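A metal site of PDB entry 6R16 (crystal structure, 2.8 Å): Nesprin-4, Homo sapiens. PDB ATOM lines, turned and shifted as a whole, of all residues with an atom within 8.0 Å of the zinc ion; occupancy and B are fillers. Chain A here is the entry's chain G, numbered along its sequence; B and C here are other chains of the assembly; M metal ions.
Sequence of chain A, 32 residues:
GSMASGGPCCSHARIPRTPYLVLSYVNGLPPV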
ATOM      1  N   PRO A   8      -3.291   1.879 -13.323  1.00  0.00           N
ATOM      2  CA  PRO A   8      -4.511   1.686 -12.527  1.00  0.00           C
ATOM      3  C   PRO A   8      -5.465   2.867 -12.693  1.00  0.00           C
ATOM      4  O   PRO A   8      -5.059   3.989 -12.988  1.00  0.00           O
ATOM      5  CB  PRO A   8      -3.991   1.582 -11.090  1.00  0.00           C
ATOM      6  CG  PRO A   8      -2.546   1.195 -11.228  1.00  0.00           C
ATOM      7  CD  PRO A   8      -2.077   1.869 -12.481  1.00  0.00           C
ATOM      8  N   CYS A   9      -6.749   2.589 -12.468  1.00  0.00           N
ATOM      9  CA  CYS A   9      -7.769   3.618 -12.636  1.00  0.00           C
ATOM     10  C   CYS A   9      -7.935   4.458 -11.381  1.00  0.00           C
ATOM     11  O   CYS A   9      -8.038   5.687 -11.466  1.00  0.00           O
ATOM     12  CB  CYS A   9      -9.102   2.965 -13.019  1.00  0.00           C
ATOM     13  SG  CYS A   9      -9.537   1.545 -11.999  1.00  0.00           S
ATOM     14  N   CYS A  10      -7.948   3.827 -10.205  1.00  0.00           N
ATOM     15  CA  CYS A  10      -8.078   4.536  -8.943  1.00  0.00           C
ATOM     16  C   CYS A  10      -7.226   3.833  -7.896  1.00  0.00           C
ATOM     17  O   CYS A  10      -6.618   2.792  -8.160  1.00  0.00           O
ATOM     18  CB  CYS A  10      -9.539   4.624  -8.488  1.00  0.00           C
ATOM     19  SG  CYS A  10     -10.320   3.026  -8.148  1.00  0.00           S
ATOM     20  N   SER A  11      -7.184   4.408  -6.697  1.00  0.00           N
ATOM     21  CA  SER A  11      -6.392   3.815  -5.626  1.00  0.00           C
ATOM     22  C   SER A  11      -7.026   2.528  -5.110  1.00  0.00           C
ATOM     23  O   SER A  11      -6.320   1.659  -4.589  1.00  0.00           O
ATOM     24  CB  SER A  11      -6.230   4.819  -4.475  1.00  0.00           C
ATOM     25  OG  SER A  11      -7.479   5.171  -3.923  1.00  0.00           O
ATOM     26  N   HIS A  12      -8.343   2.382  -5.252  1.00  0.00           N
ATOM     27  CA  HIS A  12      -9.041   1.191  -4.809  1.00  0.00           C
ATOM     28  C   HIS A  12      -9.087   0.099  -5.878  1.00  0.00           C
ATOM     29  O   HIS A  12      -9.765  -0.912  -5.670  1.00  0.00           O
ATOM     30  CB  HIS A  12     -10.478   1.542  -4.389  1.00  0.00           C
ATOM     31  CG  HIS A  12     -10.553   2.399  -3.169  1.00  0.00           C
ATOM     32  ND1 HIS A  12     -10.331   1.907  -1.892  1.00  0.00           N
ATOM     33  CD2 HIS A  12     -10.840   3.711  -3.015  1.00  0.00           C
ATOM     34  CE1 HIS A  12     -10.466   2.877  -1.014  1.00  0.00           C
ATOM     35  NE2 HIS A  12     -10.775   3.989  -1.661  1.00  0.00           N
ATOM     36  N   ALA A  13      -8.401   0.274  -6.998  1.00  0.00           N
ATOM     37  CA  ALA A  13      -8.486  -0.695  -8.078  1.00  0.00           C
ATOM     38  C   ALA A  13      -7.772  -1.988  -7.699  1.00  0.00           C
ATOM     39  O   ALA A  13      -6.601  -1.973  -7.304  1.00  0.00           O
ATOM     40  CB  ALA A  13      -7.888  -0.126  -9.354  1.00  0.00           C
ATOM     41  N   ARG A  14      -8.485  -3.106  -7.817  1.00  0.00           N
ATOM     42  CA  ARG A  14      -7.961  -4.422  -7.464  1.00  0.00           C
ATOM     43  C   ARG A  14      -7.432  -5.101  -8.721  1.00  0.00           C
ATOM     44  O   ARG A  14      -8.118  -5.905  -9.360  1.00  0.00           O
ATOM     45  CB  ARG A  14      -9.025  -5.256  -6.754  1.00  0.00           C
ATOM     46  CG  ARG A  14      -8.467  -6.536  -6.131  1.00  0.00           C
ATOM     47  CD  ARG A  14      -7.736  -6.234  -4.830  1.00  0.00           C
ATOM     48  NE  ARG A  14      -8.608  -5.623  -3.824  1.00  0.00           N
ATOM     49  CZ  ARG A  14      -9.117  -6.277  -2.791  1.00  0.00           C
ATOM     50  NH1 ARG A  14      -8.853  -7.571  -2.617  1.00  0.00           N
ATOM     51  NH2 ARG A  14      -9.900  -5.649  -1.922  1.00  0.00           N
ATOM     52  N   CYS B   9     -14.548  -4.204  -6.057  1.00  0.00           N
ATOM     53  CA  CYS B   9     -13.597  -3.384  -5.327  1.00  0.00           C
ATOM     54  C   CYS B   9     -13.409  -2.006  -5.949  1.00  0.00           C
ATOM     55  O   CYS B   9     -12.618  -1.212  -5.421  1.00  0.00           O
ATOM     56  CB  CYS B   9     -12.238  -4.090  -5.239  1.00  0.00           C
ATOM     57  SG  CYS B   9     -12.264  -5.628  -4.297  1.00  0.00           S
ATOM     58  N   CYS B  10     -14.107  -1.698  -7.036  1.00  0.00           N
ATOM     59  CA  CYS B  10     -13.981  -0.409  -7.689  1.00  0.00           C
ATOM     60  C   CYS B  10     -15.195  -0.189  -8.584  1.00  0.00           C
ATOM     61  O   CYS B  10     -15.989  -1.109  -8.824  1.00  0.00           O
ATOM     62  CB  CYS B  10     -12.682  -0.314  -8.500  1.00  0.00           C
ATOM     63  SG  CYS B  10     -12.317   1.323  -9.142  1.00  0.00           S
ATOM     64  N   SER B  11     -15.334   1.041  -9.083  1.00  0.00           N
ATOM     65  CA  SER B  11     -16.428   1.388  -9.970  1.00  0.00           C
ATOM     66  C   SER B  11     -15.983   1.644 -11.410  1.00  0.00           C
ATOM     67  O   SER B  11     -16.846   1.773 -12.280  1.00  0.00           O
ATOM     68  CB  SER B  11     -17.168   2.633  -9.452  1.00  0.00           C
ATOM     69  OG  SER B  11     -17.880   2.334  -8.265  1.00  0.00           O
ATOM     70  N   HIS B  12     -14.683   1.710 -11.669  1.00  0.00           N
ATOM     71  CA  HIS B  12     -14.195   1.879 -13.036  1.00  0.00           C
ATOM     72  C   HIS B  12     -14.204   0.534 -13.752  1.00  0.00           C
ATOM     73  O   HIS B  12     -13.624  -0.438 -13.270  1.00  0.00           O
ATOM     74  CB  HIS B  12     -12.780   2.454 -13.017  1.00  0.00           C
ATOM     75  CG  HIS B  12     -12.683   3.778 -12.318  1.00  0.00           C
ATOM     76  ND1 HIS B  12     -12.076   3.917 -11.085  1.00  0.00           N
ATOM     77  CD2 HIS B  12     -13.113   5.018 -12.668  1.00  0.00           C
ATOM     78  CE1 HIS B  12     -12.143   5.186 -10.703  1.00  0.00           C
ATOM     79  NE2 HIS B  12     -12.761   5.869 -11.652  1.00  0.00           N
ATOM     80  N   ALA B  13     -14.849   0.488 -14.905  1.00  0.00           N
ATOM     81  CA  ALA B  13     -14.917  -0.749 -15.665  1.00  0.00           C
ATOM     82  C   ALA B  13     -13.551  -1.105 -16.259  1.00  0.00           C
ATOM     83  O   ALA B  13     -12.796  -0.228 -16.683  1.00  0.00           O
ATOM     84  CB  ALA B  13     -15.949  -0.638 -16.787  1.00  0.00           C
ATOM     85  N   ARG B  14     -13.237  -2.394 -16.273  1.00  0.00           N
ATOM     86  CA  ARG B  14     -11.989  -2.851 -16.885  1.00  0.00           C
ATOM     87  C   ARG B  14     -12.055  -2.749 -18.396  1.00  0.00           C
ATOM     88  O   ARG B  14     -11.039  -2.469 -19.048  1.00  0.00           O
ATOM     89  CB  ARG B  14     -11.671  -4.276 -16.445  1.00  0.00           C
ATOM     90  CG  ARG B  14     -10.199  -4.644 -16.537  1.00  0.00           C
ATOM     91  CD  ARG B  14      -9.337  -3.729 -15.664  1.00  0.00           C
ATOM     92  NE  ARG B  14      -9.663  -3.847 -14.248  1.00  0.00           N
ATOM     93  CZ  ARG B  14      -9.017  -4.638 -13.392  1.00  0.00           C
ATOM     94  NH1 ARG B  14      -8.011  -5.394 -13.808  1.00  0.00           N
ATOM     95  NH2 ARG B  14      -9.385  -4.670 -12.118  1.00  0.00           N
ATOM     96  N   PRO C  65     -14.396  -5.272 -11.452  1.00  0.00           N
ATOM     97  CA  PRO C  65     -15.383  -4.682 -12.354  1.00  0.00           C
ATOM     98  C   PRO C  65     -15.007  -4.939 -13.801  1.00  0.00           C
ATOM     99  O   PRO C  65     -13.885  -4.663 -14.226  1.00  0.00           O
ATOM    100  CB  PRO C  65     -15.336  -3.189 -12.010  1.00  0.00           C
ATOM    101  CG  PRO C  65     -13.970  -2.987 -11.432  1.00  0.00           C
ATOM    102  CD  PRO C  65     -13.646  -4.250 -10.687  1.00  0.00           C
HETATM  103 ZN    ZN M   1     -10.812   2.480 -10.324  1.00  0.00          ZN
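Of the 14 residues printed, 4 come within 4 Å of the zinc ion.
Along chain A the residues within 4 Å of the zinc ion span positions 9 to 10.
The nearest printed residue that does not touch the zinc ion is Ala 13 of chain A (4.04 Å).
SG of Cys 10 of chain A sits close to N of Ala 13 of chain A.
The side-chain sulfur of Cys 10 of chain A lies close to the backbone NH of His 12 of chain A (3.6 Å).
The zinc ion is bound by a ring nitrogen (ND1) of His 12 of chain B, the side-chain sulfur (SG) of Cys 10 of chain B, the side-chain sulfur (SG) of Cys 10 of chain A and the side-chain sulfur (SG) of Cys 9 of chain A.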
